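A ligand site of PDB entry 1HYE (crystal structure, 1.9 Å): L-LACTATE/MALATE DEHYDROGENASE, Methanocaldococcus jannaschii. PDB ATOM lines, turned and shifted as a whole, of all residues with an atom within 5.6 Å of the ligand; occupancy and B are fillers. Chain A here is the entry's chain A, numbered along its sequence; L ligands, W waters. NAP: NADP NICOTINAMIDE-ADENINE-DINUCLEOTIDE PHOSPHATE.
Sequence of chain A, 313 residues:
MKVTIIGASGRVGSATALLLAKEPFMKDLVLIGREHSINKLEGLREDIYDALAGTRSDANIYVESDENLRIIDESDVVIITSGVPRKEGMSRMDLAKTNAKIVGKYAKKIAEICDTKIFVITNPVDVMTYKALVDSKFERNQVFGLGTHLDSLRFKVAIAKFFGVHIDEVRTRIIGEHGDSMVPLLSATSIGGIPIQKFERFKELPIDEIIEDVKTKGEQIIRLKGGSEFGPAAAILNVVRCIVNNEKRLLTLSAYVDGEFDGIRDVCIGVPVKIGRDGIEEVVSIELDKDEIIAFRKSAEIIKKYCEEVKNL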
ATOM      1  N   ILE A   6      26.974 -19.188 -19.613  1.00  0.00           N
ATOM      2  CA  ILE A   6      26.431 -19.526 -18.306  1.00  0.00           C
ATOM      3  C   ILE A   6      25.106 -18.784 -18.236  1.00  0.00           C
ATOM      4  O   ILE A   6      25.064 -17.560 -18.215  1.00  0.00           O
ATOM      5  CB  ILE A   6      27.372 -19.076 -17.183  1.00  0.00           C
ATOM      6  CG1 ILE A   6      28.725 -19.776 -17.346  1.00  0.00           C
ATOM      7  CG2 ILE A   6      26.748 -19.390 -15.836  1.00  0.00           C
ATOM      8  CD1 ILE A   6      29.757 -19.371 -16.324  1.00  0.00           C
ATOM      9  N   GLY A   7      24.014 -19.552 -18.231  1.00  0.00           N
ATOM     10  CA  GLY A   7      22.695 -18.954 -18.218  1.00  0.00           C
ATOM     11  C   GLY A   7      22.017 -19.300 -19.526  1.00  0.00           C
ATOM     12  O   GLY A   7      21.046 -18.654 -19.938  1.00  0.00           O
ATOM     13  N   ALA A   8      22.522 -20.339 -20.190  1.00  0.00           N
ATOM     14  CA  ALA A   8      21.979 -20.805 -21.460  1.00  0.00           C
ATOM     15  C   ALA A   8      20.526 -21.311 -21.399  1.00  0.00           C
ATOM     16  O   ALA A   8      19.860 -21.406 -22.431  1.00  0.00           O
ATOM     17  CB  ALA A   8      22.870 -21.917 -22.031  1.00  0.00           C
ATOM     18  N   SER A   9      20.045 -21.639 -20.208  1.00  0.00           N
ATOM     19  CA  SER A   9      18.670 -22.142 -20.087  1.00  0.00           C
ATOM     20  C   SER A   9      17.638 -21.023 -20.161  1.00  0.00           C
ATOM     21  O   SER A   9      16.442 -21.279 -20.322  1.00  0.00           O
ATOM     22  CB  SER A   9      18.485 -22.891 -18.758  1.00  0.00           C
ATOM     23  OG  SER A   9      18.528 -21.992 -17.661  1.00  0.00           O
ATOM     24  N   GLY A  10      18.101 -19.787 -20.049  1.00  0.00           N
ATOM     25  CA  GLY A  10      17.221 -18.635 -20.094  1.00  0.00           C
ATOM     26  C   GLY A  10      16.910 -18.165 -21.507  1.00  0.00           C
ATOM     27  O   GLY A  10      17.457 -18.685 -22.462  1.00  0.00           O
ATOM     28  N   ARG A  11      16.043 -17.169 -21.609  1.00  0.00           N
ATOM     29  CA  ARG A  11      15.629 -16.643 -22.913  1.00  0.00           C
ATOM     30  C   ARG A  11      16.753 -16.108 -23.772  1.00  0.00           C
ATOM     31  O   ARG A  11      16.906 -16.524 -24.925  1.00  0.00           O
ATOM     32  CB  ARG A  11      14.566 -15.568 -22.718  1.00  0.00           C
ATOM     33  CG  ARG A  11      13.382 -16.039 -21.877  1.00  0.00           C
ATOM     34  CD  ARG A  11      12.379 -14.914 -21.645  1.00  0.00           C
ATOM     35  NE  ARG A  11      11.272 -15.344 -20.783  1.00  0.00           N
ATOM     36  CZ  ARG A  11      10.398 -16.295 -21.102  1.00  0.00           C
ATOM     37  NH1 ARG A  11      10.492 -16.925 -22.262  1.00  0.00           N
ATOM     38  NH2 ARG A  11       9.420 -16.611 -20.265  1.00  0.00           N
ATOM     39  N   VAL A  12      17.541 -15.161 -23.256  1.00  0.00           N
ATOM     40  CA  VAL A  12      18.608 -14.613 -24.063  1.00  0.00           C
ATOM     41  C   VAL A  12      19.753 -15.629 -24.230  1.00  0.00           C
ATOM     42  O   VAL A  12      20.408 -15.673 -25.258  1.00  0.00           O
ATOM     43  CB  VAL A  12      19.148 -13.274 -23.496  1.00  0.00           C
ATOM     44  CG1 VAL A  12      19.782 -13.490 -22.122  1.00  0.00           C
ATOM     45  CG2 VAL A  12      20.168 -12.686 -24.463  1.00  0.00           C
ATOM     46  N   GLY A  13      19.971 -16.454 -23.204  1.00  0.00           N
ATOM     47  CA  GLY A  13      21.035 -17.444 -23.282  1.00  0.00           C
ATOM     48  C   GLY A  13      20.753 -18.505 -24.338  1.00  0.00           C
ATOM     49  O   GLY A  13      21.648 -18.890 -25.097  1.00  0.00           O
ATOM     50  N   GLY A  33      24.168 -24.490 -16.734  1.00  0.00           N
ATOM     51  CA  GLY A  33      22.951 -24.109 -16.048  1.00  0.00           C
ATOM     52  C   GLY A  33      22.933 -24.802 -14.700  1.00  0.00           C
ATOM     53  O   GLY A  33      23.767 -25.671 -14.429  1.00  0.00           O
ATOM     54  N   ARG A  34      22.001 -24.415 -13.842  1.00  0.00           N
ATOM     55  CA  ARG A  34      21.911 -25.035 -12.530  1.00  0.00           C
ATOM     56  C   ARG A  34      21.416 -26.467 -12.711  1.00  0.00           C
ATOM     57  O   ARG A  34      20.849 -26.814 -13.739  1.00  0.00           O
ATOM     58  CB  ARG A  34      20.971 -24.227 -11.626  1.00  0.00           C
ATOM     59  CG  ARG A  34      21.605 -22.946 -11.102  1.00  0.00           C
ATOM     60  CD  ARG A  34      20.766 -22.268 -10.029  1.00  0.00           C
ATOM     61  NE  ARG A  34      19.532 -21.693 -10.568  1.00  0.00           N
ATOM     62  CZ  ARG A  34      18.634 -21.031  -9.844  1.00  0.00           C
ATOM     63  NH1 ARG A  34      17.548 -20.540 -10.413  1.00  0.00           N
ATOM     64  NH2 ARG A  34      18.827 -20.866  -8.540  1.00  0.00           N
ATOM     65  N   HIS A  36      18.846 -28.137 -11.808  1.00  0.00           N
ATOM     66  CA  HIS A  36      17.457 -28.353 -12.194  1.00  0.00           C
ATOM     67  C   HIS A  36      17.153 -28.001 -13.645  1.00  0.00           C
ATOM     68  O   HIS A  36      16.047 -28.218 -14.125  1.00  0.00           O
ATOM     69  CB  HIS A  36      16.515 -27.577 -11.264  1.00  0.00           C
ATOM     70  CG  HIS A  36      16.637 -26.091 -11.387  1.00  0.00           C
ATOM     71  ND1 HIS A  36      15.841 -25.224 -10.656  1.00  0.00           N
ATOM     72  CD2 HIS A  36      17.423 -25.312 -12.157  1.00  0.00           C
ATOM     73  CE1 HIS A  36      16.132 -23.980 -10.980  1.00  0.00           C
ATOM     74  NE2 HIS A  36      17.089 -24.005 -11.883  1.00  0.00           N
ATOM     75  N   SER A  37      18.146 -27.462 -14.332  1.00  0.00           N
ATOM     76  CA  SER A  37      17.982 -27.050 -15.731  1.00  0.00           C
ATOM     77  C   SER A  37      18.567 -28.002 -16.777  1.00  0.00           C
ATOM     78  O   SER A  37      18.399 -27.789 -17.968  1.00  0.00           O
ATOM     79  CB  SER A  37      18.573 -25.658 -15.920  1.00  0.00           C
ATOM     80  OG  SER A  37      17.746 -24.676 -15.273  1.00  0.00           O
ATOM     81  N   ASP A  66      26.412 -26.187 -13.197  1.00  0.00           N
ATOM     82  CA  ASP A  66      27.399 -25.226 -12.713  1.00  0.00           C
ATOM     83  C   ASP A  66      28.143 -25.677 -11.442  1.00  0.00           C
ATOM     84  O   ASP A  66      28.784 -24.863 -10.786  1.00  0.00           O
ATOM     85  CB  ASP A  66      26.736 -23.867 -12.478  1.00  0.00           C
ATOM     86  CG  ASP A  66      25.684 -23.907 -11.386  1.00  0.00           C
ATOM     87  OD1 ASP A  66      25.451 -24.989 -10.806  1.00  0.00           O
ATOM     88  OD2 ASP A  66      25.093 -22.844 -11.103  1.00  0.00           O
ATOM     89  N   THR A  81      24.723 -14.757 -18.782  1.00  0.00           N
ATOM     90  CA  THR A  81      23.375 -14.231 -18.961  1.00  0.00           C
ATOM     91  C   THR A  81      22.474 -14.667 -17.799  1.00  0.00           C
ATOM     92  O   THR A  81      21.271 -14.434 -17.836  1.00  0.00           O
ATOM     93  CB  THR A  81      22.717 -14.727 -20.285  1.00  0.00           C
ATOM     94  OG1 THR A  81      22.526 -16.149 -20.235  1.00  0.00           O
ATOM     95  CG2 THR A  81      23.587 -14.398 -21.494  1.00  0.00           C
ATOM     96  N   SER A  82      23.066 -15.299 -16.798  1.00  0.00           N
ATOM     97  CA  SER A  82      22.308 -15.747 -15.625  1.00  0.00           C
ATOM     98  C   SER A  82      21.935 -14.543 -14.781  1.00  0.00           C
ATOM     99  O   SER A  82      22.751 -13.652 -14.560  1.00  0.00           O
ATOM    100  CB  SER A  82      23.134 -16.703 -14.761  1.00  0.00           C
ATOM    101  OG  SER A  82      23.517 -17.863 -15.469  1.00  0.00           O
ATOM    102  N   GLY A  83      20.709 -14.535 -14.282  1.00  0.00           N
ATOM    103  CA  GLY A  83      20.272 -13.436 -13.442  1.00  0.00           C
ATOM    104  C   GLY A  83      18.767 -13.272 -13.476  1.00  0.00           C
ATOM    105  O   GLY A  83      18.098 -13.777 -14.378  1.00  0.00           O
ATOM    106  N   VAL A  84      18.240 -12.588 -12.477  1.00  0.00           N
ATOM    107  CA  VAL A  84      16.799 -12.354 -12.417  1.00  0.00           C
ATOM    108  C   VAL A  84      16.512 -11.091 -13.237  1.00  0.00           C
ATOM    109  O   VAL A  84      17.115 -10.039 -13.006  1.00  0.00           O
ATOM    110  CB  VAL A  84      16.325 -12.147 -10.974  1.00  0.00           C
ATOM    111  CG1 VAL A  84      14.817 -11.973 -10.947  1.00  0.00           C
ATOM    112  CG2 VAL A  84      16.742 -13.331 -10.116  1.00  0.00           C
ATOM    113  N   PRO A  85      15.599 -11.192 -14.204  1.00  0.00           N
ATOM    114  CA  PRO A  85      15.253 -10.058 -15.057  1.00  0.00           C
ATOM    115  C   PRO A  85      14.444  -8.989 -14.305  1.00  0.00           C
ATOM    116  O   PRO A  85      14.070  -9.175 -13.144  1.00  0.00           O
ATOM    117  CB  PRO A  85      14.452 -10.714 -16.174  1.00  0.00           C
ATOM    118  CG  PRO A  85      13.721 -11.793 -15.449  1.00  0.00           C
ATOM    119  CD  PRO A  85      14.807 -12.381 -14.572  1.00  0.00           C
ATOM    120  N   ARG A  86      14.211  -7.868 -14.987  1.00  0.00           N
ATOM    121  CA  ARG A  86      13.467  -6.751 -14.422  1.00  0.00           C
ATOM    122  C   ARG A  86      12.236  -7.185 -13.624  1.00  0.00           C
ATOM    123  O   ARG A  86      11.187  -7.481 -14.186  1.00  0.00           O
ATOM    124  CB  ARG A  86      13.043  -5.790 -15.546  1.00  0.00           C
ATOM    125  CG  ARG A  86      12.150  -6.405 -16.636  1.00  0.00           C
ATOM    126  CD  ARG A  86      12.827  -7.558 -17.382  1.00  0.00           C
ATOM    127  NE  ARG A  86      14.132  -7.184 -17.924  1.00  0.00           N
ATOM    128  CZ  ARG A  86      14.928  -8.008 -18.596  1.00  0.00           C
ATOM    129  NH1 ARG A  86      16.095  -7.573 -19.049  1.00  0.00           N
ATOM    130  NH2 ARG A  86      14.552  -9.260 -18.826  1.00  0.00           N
ATOM    131  N   ASN A  99      21.536  -9.784  -8.265  1.00  0.00           N
ATOM    132  CA  ASN A  99      22.329 -10.311  -9.362  1.00  0.00           C
ATOM    133  C   ASN A  99      23.821 -10.208  -9.135  1.00  0.00           C
ATOM    134  O   ASN A  99      24.596 -10.959  -9.729  1.00  0.00           O
ATOM    135  CB  ASN A  99      21.924  -9.629 -10.679  1.00  0.00           C
ATOM    136  CG  ASN A  99      20.549 -10.066 -11.151  1.00  0.00           C
ATOM    137  OD1 ASN A  99      20.131 -11.197 -10.909  1.00  0.00           O
ATOM    138  ND2 ASN A  99      19.845  -9.182 -11.841  1.00  0.00           N
ATOM    139  N   ILE A 102      24.985 -13.428  -7.909  1.00  0.00           N
ATOM    140  CA  ILE A 102      24.989 -14.474  -8.934  1.00  0.00           C
ATOM    141  C   ILE A 102      26.215 -14.327  -9.834  1.00  0.00           C
ATOM    142  O   ILE A 102      27.031 -15.232  -9.942  1.00  0.00           O
ATOM    143  CB  ILE A 102      23.698 -14.416  -9.799  1.00  0.00           C
ATOM    144  CG1 ILE A 102      22.480 -14.743  -8.917  1.00  0.00           C
ATOM    145  CG2 ILE A 102      23.787 -15.401 -10.971  1.00  0.00           C
ATOM    146  CD1 ILE A 102      21.149 -14.309  -9.516  1.00  0.00           C
ATOM    147  N   TYR A 106      29.991 -16.636 -10.140  1.00  0.00           N
ATOM    148  CA  TYR A 106      30.457 -17.237 -11.380  1.00  0.00           C
ATOM    149  C   TYR A 106      31.795 -16.666 -11.828  1.00  0.00           C
ATOM    150  O   TYR A 106      32.638 -17.393 -12.350  1.00  0.00           O
ATOM    151  CB  TYR A 106      29.411 -17.032 -12.502  1.00  0.00           C
ATOM    152  CG  TYR A 106      28.206 -17.949 -12.388  1.00  0.00           C
ATOM    153  CD1 TYR A 106      26.904 -17.463 -12.574  1.00  0.00           C
ATOM    154  CD2 TYR A 106      28.363 -19.304 -12.076  1.00  0.00           C
ATOM    155  CE1 TYR A 106      25.802 -18.303 -12.462  1.00  0.00           C
ATOM    156  CE2 TYR A 106      27.244 -20.162 -11.967  1.00  0.00           C
ATOM    157  CZ  TYR A 106      25.968 -19.638 -12.151  1.00  0.00           C
ATOM    158  OH  TYR A 106      24.873 -20.467 -12.044  1.00  0.00           O
ATOM    159  N   ILE A 121      26.034  -9.967 -19.668  1.00  0.00           N
ATOM    160  CA  ILE A 121      24.765  -9.515 -20.237  1.00  0.00           C
ATOM    161  C   ILE A 121      23.725  -9.214 -19.156  1.00  0.00           C
ATOM    162  O   ILE A 121      22.815  -8.406 -19.369  1.00  0.00           O
ATOM    163  CB  ILE A 121      24.185 -10.584 -21.199  1.00  0.00           C
ATOM    164  CG1 ILE A 121      25.270 -11.064 -22.180  1.00  0.00           C
ATOM    165  CG2 ILE A 121      22.984 -10.025 -21.938  1.00  0.00           C
ATOM    166  CD1 ILE A 121      25.850  -9.959 -23.061  1.00  0.00           C
ATOM    167  N   THR A 122      23.852  -9.864 -17.996  1.00  0.00           N
ATOM    168  CA  THR A 122      22.866  -9.655 -16.931  1.00  0.00           C
ATOM    169  C   THR A 122      22.827  -8.221 -16.411  1.00  0.00           C
ATOM    170  O   THR A 122      23.858  -7.549 -16.275  1.00  0.00           O
ATOM    171  CB  THR A 122      23.059 -10.710 -15.778  1.00  0.00           C
ATOM    172  OG1 THR A 122      23.076 -10.072 -14.502  1.00  0.00           O
ATOM    173  CG2 THR A 122      24.291 -11.548 -16.001  1.00  0.00           C
ATOM    174  N   ASN A 123      21.617  -7.738 -16.160  1.00  0.00           N
ATOM    175  CA  ASN A 123      21.390  -6.356 -15.683  1.00  0.00           C
ATOM    176  C   ASN A 123      21.430  -6.220 -14.166  1.00  0.00           C
ATOM    177  O   ASN A 123      21.189  -7.187 -13.429  1.00  0.00           O
ATOM    178  CB  ASN A 123      20.039  -5.839 -16.176  1.00  0.00           C
ATOM    179  CG  ASN A 123      20.053  -5.449 -17.642  1.00  0.00           C
ATOM    180  OD1 ASN A 123      21.019  -4.866 -18.118  1.00  0.00           O
ATOM    181  ND2 ASN A 123      18.962  -5.725 -18.343  1.00  0.00           N
ATOM    182  N   VAL A 125      23.566  -4.231 -16.308  1.00  0.00           N
ATOM    183  CA  VAL A 125      24.814  -4.595 -16.971  1.00  0.00           C
ATOM    184  C   VAL A 125      26.091  -3.839 -16.594  1.00  0.00           C
ATOM    185  O   VAL A 125      27.152  -4.452 -16.430  1.00  0.00           O
ATOM    186  CB  VAL A 125      24.625  -4.611 -18.521  1.00  0.00           C
ATOM    187  CG1 VAL A 125      24.457  -3.217 -19.068  1.00  0.00           C
ATOM    188  CG2 VAL A 125      25.806  -5.337 -19.175  1.00  0.00           C
ATOM    189  N   LEU A 146      27.629  -5.917 -22.525  1.00  0.00           N
ATOM    190  CA  LEU A 146      26.915  -5.430 -23.708  1.00  0.00           C
ATOM    191  C   LEU A 146      26.744  -3.906 -23.686  1.00  0.00           C
ATOM    192  O   LEU A 146      26.832  -3.232 -24.711  1.00  0.00           O
ATOM    193  CB  LEU A 146      25.558  -6.112 -23.839  1.00  0.00           C
ATOM    194  CG  LEU A 146      24.797  -5.871 -25.151  1.00  0.00           C
ATOM    195  CD1 LEU A 146      25.628  -6.279 -26.349  1.00  0.00           C
ATOM    196  CD2 LEU A 146      23.485  -6.665 -25.128  1.00  0.00           C
ATOM    197  N   GLY A 147      26.477  -3.356 -22.507  1.00  0.00           N
ATOM    198  CA  GLY A 147      26.320  -1.914 -22.366  1.00  0.00           C
ATOM    199  C   GLY A 147      25.277  -1.258 -23.272  1.00  0.00           C
ATOM    200  O   GLY A 147      24.142  -1.726 -23.369  1.00  0.00           O
ATOM    201  N   LEU A 150      23.487  -2.151 -28.267  1.00  0.00           N
ATOM    202  CA  LEU A 150      22.198  -2.320 -28.939  1.00  0.00           C
ATOM    203  C   LEU A 150      21.399  -1.003 -28.892  1.00  0.00           C
ATOM    204  O   LEU A 150      20.660  -0.684 -29.824  1.00  0.00           O
ATOM    205  CB  LEU A 150      21.393  -3.450 -28.296  1.00  0.00           C
ATOM    206  CG  LEU A 150      19.989  -3.740 -28.877  1.00  0.00           C
ATOM    207  CD1 LEU A 150      20.092  -4.000 -30.377  1.00  0.00           C
ATOM    208  CD2 LEU A 150      19.376  -4.934 -28.171  1.00  0.00           C
ATOM    209  N   HIS A 178      23.227   1.869 -19.294  1.00  0.00           N
ATOM    210  CA  HIS A 178      22.231   1.175 -20.096  1.00  0.00           C
ATOM    211  C   HIS A 178      20.997   1.294 -19.202  1.00  0.00           C
ATOM    212  O   HIS A 178      20.623   0.368 -18.499  1.00  0.00           O
ATOM    213  CB  HIS A 178      22.599  -0.303 -20.287  1.00  0.00           C
ATOM    214  CG  HIS A 178      21.525  -1.111 -20.950  1.00  0.00           C
ATOM    215  ND1 HIS A 178      21.010  -0.786 -22.189  1.00  0.00           N
ATOM    216  CD2 HIS A 178      20.870  -2.222 -20.547  1.00  0.00           C
ATOM    217  CE1 HIS A 178      20.079  -1.678 -22.514  1.00  0.00           C
ATOM    218  NE2 HIS A 178      19.982  -2.550 -21.535  1.00  0.00           N
ATOM    219  N   GLU A 219      15.694  -3.077 -25.253  1.00  0.00           N
ATOM    220  CA  GLU A 219      16.073  -4.483 -25.240  1.00  0.00           C
ATOM    221  C   GLU A 219      15.169  -5.348 -26.102  1.00  0.00           C
ATOM    222  O   GLU A 219      15.256  -6.579 -26.075  1.00  0.00           O
ATOM    223  CB  GLU A 219      16.088  -5.019 -23.807  1.00  0.00           C
ATOM    224  CG  GLU A 219      16.979  -4.237 -22.866  1.00  0.00           C
ATOM    225  CD  GLU A 219      17.268  -4.964 -21.569  1.00  0.00           C
ATOM    226  OE1 GLU A 219      16.516  -5.905 -21.215  1.00  0.00           O
ATOM    227  OE2 GLU A 219      18.255  -4.600 -20.896  1.00  0.00           O
ATOM    228  N   PRO A 232      18.903  -8.562 -28.761  1.00  0.00           N
ATOM    229  CA  PRO A 232      20.035  -8.838 -27.869  1.00  0.00           C
ATOM    230  C   PRO A 232      20.968  -9.948 -28.355  1.00  0.00           C
ATOM    231  O   PRO A 232      22.187  -9.798 -28.327  1.00  0.00           O
ATOM    232  CB  PRO A 232      19.345  -9.180 -26.556  1.00  0.00           C
ATOM    233  CG  PRO A 232      18.126  -8.301 -26.589  1.00  0.00           C
ATOM    234  CD  PRO A 232      17.644  -8.494 -28.003  1.00  0.00           C
HETATM  235  PA  NAP L   1      15.170 -15.583 -17.953  1.00  0.00           P
HETATM  236  O1A NAP L   1      13.692 -15.842 -17.615  1.00  0.00           O
HETATM  237  O2A NAP L   1      15.335 -16.073 -19.261  1.00  0.00           O
HETATM  238  O5B NAP L   1      16.174 -16.561 -17.155  1.00  0.00           O
HETATM  239  C5B NAP L   1      17.592 -16.445 -17.148  1.00  0.00           C
HETATM  240  C4B NAP L   1      17.952 -17.706 -16.595  1.00  0.00           C
HETATM  241  O4B NAP L   1      18.559 -17.146 -15.380  1.00  0.00           O
HETATM  242  C3B NAP L   1      18.371 -19.074 -16.225  1.00  0.00           C
HETATM  243  O3B NAP L   1      19.708 -19.292 -16.975  1.00  0.00           O
HETATM  244  C2B NAP L   1      18.520 -19.248 -14.868  1.00  0.00           C
HETATM  245  O2B NAP L   1      18.997 -20.411 -14.350  1.00  0.00           O
HETATM  246  C1B NAP L   1      19.343 -18.086 -14.560  1.00  0.00           C
HETATM  247  N9A NAP L   1      19.190 -17.739 -13.032  1.00  0.00           N
HETATM  248  C8A NAP L   1      18.163 -17.148 -12.369  1.00  0.00           C
HETATM  249  N7A NAP L   1      18.360 -17.071 -11.120  1.00  0.00           N
HETATM  250  C5A NAP L   1      19.587 -17.673 -10.878  1.00  0.00           C
HETATM  251  C6A NAP L   1      20.380 -17.911  -9.702  1.00  0.00           C
HETATM  252  N6A NAP L   1      19.984 -17.547  -8.482  1.00  0.00           N
HETATM  253  N1A NAP L   1      21.591 -18.525  -9.843  1.00  0.00           N
HETATM  254  C2A NAP L   1      22.035 -18.905 -11.075  1.00  0.00           C
HETATM  255  N3A NAP L   1      21.345 -18.739 -12.232  1.00  0.00           N
HETATM  256  C4A NAP L   1      20.141 -18.072 -12.037  1.00  0.00           C
HETATM  257  O3  NAP L   1      15.721 -14.123 -18.101  1.00  0.00           O
HETATM  258  PN  NAP L   1      16.383 -13.388 -19.423  1.00  0.00           P
HETATM  259  O1N NAP L   1      15.297 -12.713 -20.158  1.00  0.00           O
HETATM  260  O2N NAP L   1      17.137 -14.431 -20.213  1.00  0.00           O
HETATM  261  O5D NAP L   1      17.528 -12.387 -18.989  1.00  0.00           O
HETATM  262  C5D NAP L   1      18.657 -12.830 -18.227  1.00  0.00           C
HETATM  263  C4D NAP L   1      19.454 -11.666 -17.600  1.00  0.00           C
HETATM  264  O4D NAP L   1      20.090 -10.880 -18.590  1.00  0.00           O
HETATM  265  C3D NAP L   1      18.628 -10.658 -16.767  1.00  0.00           C
HETATM  266  O3D NAP L   1      19.326 -10.103 -15.642  1.00  0.00           O
HETATM  267  C2D NAP L   1      18.253  -9.577 -17.747  1.00  0.00           C
HETATM  268  O2D NAP L   1      18.051  -8.313 -17.178  1.00  0.00           O
HETATM  269  C1D NAP L   1      19.481  -9.590 -18.687  1.00  0.00           C
HETATM  270  N1N NAP L   1      19.152  -9.207 -20.062  1.00  0.00           N
HETATM  271  C2N NAP L   1      19.919  -8.129 -20.551  1.00  0.00           C
HETATM  272  C3N NAP L   1      19.648  -7.683 -21.898  1.00  0.00           C
HETATM  273  C7N NAP L   1      20.413  -6.572 -22.499  1.00  0.00           C
HETATM  274  O7N NAP L   1      20.203  -6.163 -23.639  1.00  0.00           O
HETATM  275  N7N NAP L   1      21.370  -5.950 -21.799  1.00  0.00           N
HETATM  276  C4N NAP L   1      18.632  -8.344 -22.631  1.00  0.00           C
HETATM  277  C5N NAP L   1      17.893  -9.375 -22.137  1.00  0.00           C
HETATM  278  C6N NAP L   1      18.146  -9.818 -20.848  1.00  0.00           C
HETATM  279  P2B NAP L   1      17.991 -21.667 -14.147  1.00  0.00           P
HETATM  280  O1X NAP L   1      17.131 -21.836 -15.278  1.00  0.00           O
HETATM  281  O2X NAP L   1      19.063 -22.597 -13.904  1.00  0.00           O
HETATM  282  O3X NAP L   1      17.222 -21.358 -12.865  1.00  0.00           O
HETATM  283  O   HOH W   1      22.926 -20.101 -14.140  1.00  0.00           O
HETATM  284  O   HOH W   2      15.136 -11.686 -22.553  1.00  0.00           O
HETATM  285  O   HOH W   3      23.107  -3.943 -22.587  1.00  0.00           O
HETATM  286  O   HOH W   4      19.632 -16.203 -20.368  1.00  0.00           O
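The side-chain hydroxyl of Ser 37 sits at hydrogen-bond distance from an oxygen (O2X) of the ligand, at 2.8 Å. OG of Ser 9 sits at hydrogen-bond distance from O1X of the ligand. O3D of the ligand sits at hydrogen-bond distance from N of Asn 123. The backbone NH (N) of Arg 11 sits at hydrogen-bond distance from an oxygen (O2A) of the ligand, 2.7 Å away. O of Gly 7 sits close to O3B of the ligand (3.3 Å). NH2 of Arg 86 lies within salt-bridge range of O1N of the ligand, 3.8 Å away. The guanidinium group of Arg 34 lies within salt-bridge range of an oxygen (O3X) of the ligand. O of Val 84 is in hydrogen-bond range of O3D of the ligand, at 3.4 Å. The backbone NH of Arg 34 sits close to an oxygen (O2X) of the ligand (3.5 Å). N of Val 12 sits at hydrogen-bond distance from O2N of the ligand (3.2 Å). An oxygen (O3X) of the ligand is in hydrogen-bond range of a ring nitrogen (NE2) of His 36 (2.8 Å). An oxygen (O2D) of the ligand is in hydrogen-bond range of the side-chain amide nitrogen of Asn 123.
OG1 of Thr 81 lies within hydrogen-bond range of O of Gly 7. The side-chain hydroxyl (OH) of Tyr 106 sits at hydrogen-bond distance from the side-chain carboxylate (OD2) of Asp 66 (2.6 Å). A ring nitrogen (ND1) of His 178 is in hydrogen-bond range of the backbone carbonyl oxygen (O) of Gly 147 (3.5 Å). NH1 of Arg 86 is in salt-bridge range of OE1 of Glu 219. The side-chain hydroxyl (OG) of Ser 82 sits at hydrogen-bond distance from the backbone carbonyl oxygen (O) of Ile 6. The side-chain amide nitrogen (ND2) of Asn 123 is in hydrogen-bond range of the side-chain carboxylate (OE2) of Glu 219. The backbone carbonyl oxygen (O) of Ile 6 is in hydrogen-bond range of the backbone NH (N) of Thr 81, 2.9 Å away. N of Gly 7 lies close to OG of Ser 82 (3.3 Å).
Gly 10 touches the ligand. O of Thr 81 touches C5D of the ligand (3.1 Å). Ser 82 touches the ligand (CB to N3A, 3.7 Å). O of Gly 83 touches O4B of the ligand, at 3.5 Å. Pro 85 touches the ligand (CA to C3D, 3.8 Å). ND2 of Asn 99 touches O3D of the ligand, 3.9 Å away. Ile 102 touches the ligand. Tyr 106 touches the ligand (OH to C2A, 3.4 Å). Ile 121 touches the ligand (O to C2N, 3.1 Å). Thr 122 touches the ligand. Leu 146 touches the ligand (CD2 to O7N, 3.6 Å). NE2 of His 178 touches N7N of the ligand, at 3.7 Å. Glu 219 touches the ligand (OE2 to C7N, 3.3 Å). CG of Pro 232 touches C4N of the ligand (3.99 Å). Hydrophobic or aromatic side chains within 4 Å of the ligand: Val 12, His 36, Ile 102, Ile 121, Leu 146, His 178 and Pro 232. Of the 32 residues printed, 24 come within 4 Å of the ligand.
Water W3 lies within hydrogen-bond range of O of Gly 147 (2.6 Å) and N7N of the ligand (2.8 Å). Water W1 lies within hydrogen-bond range of the side-chain hydroxyl (OG) of Ser 82 (2.7 Å), a nitrogen (N3A) of the ligand (2.8 Å) and the side-chain hydroxyl (OH) of Tyr 106 (2.9 Å). Water W4 lies within hydrogen-bond range of O of Gly 7 (2.9 Å), N of Gly 13 (2.9 Å), OG1 of Thr 81 (2.9 Å) and O2N of the ligand (3.1 Å).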
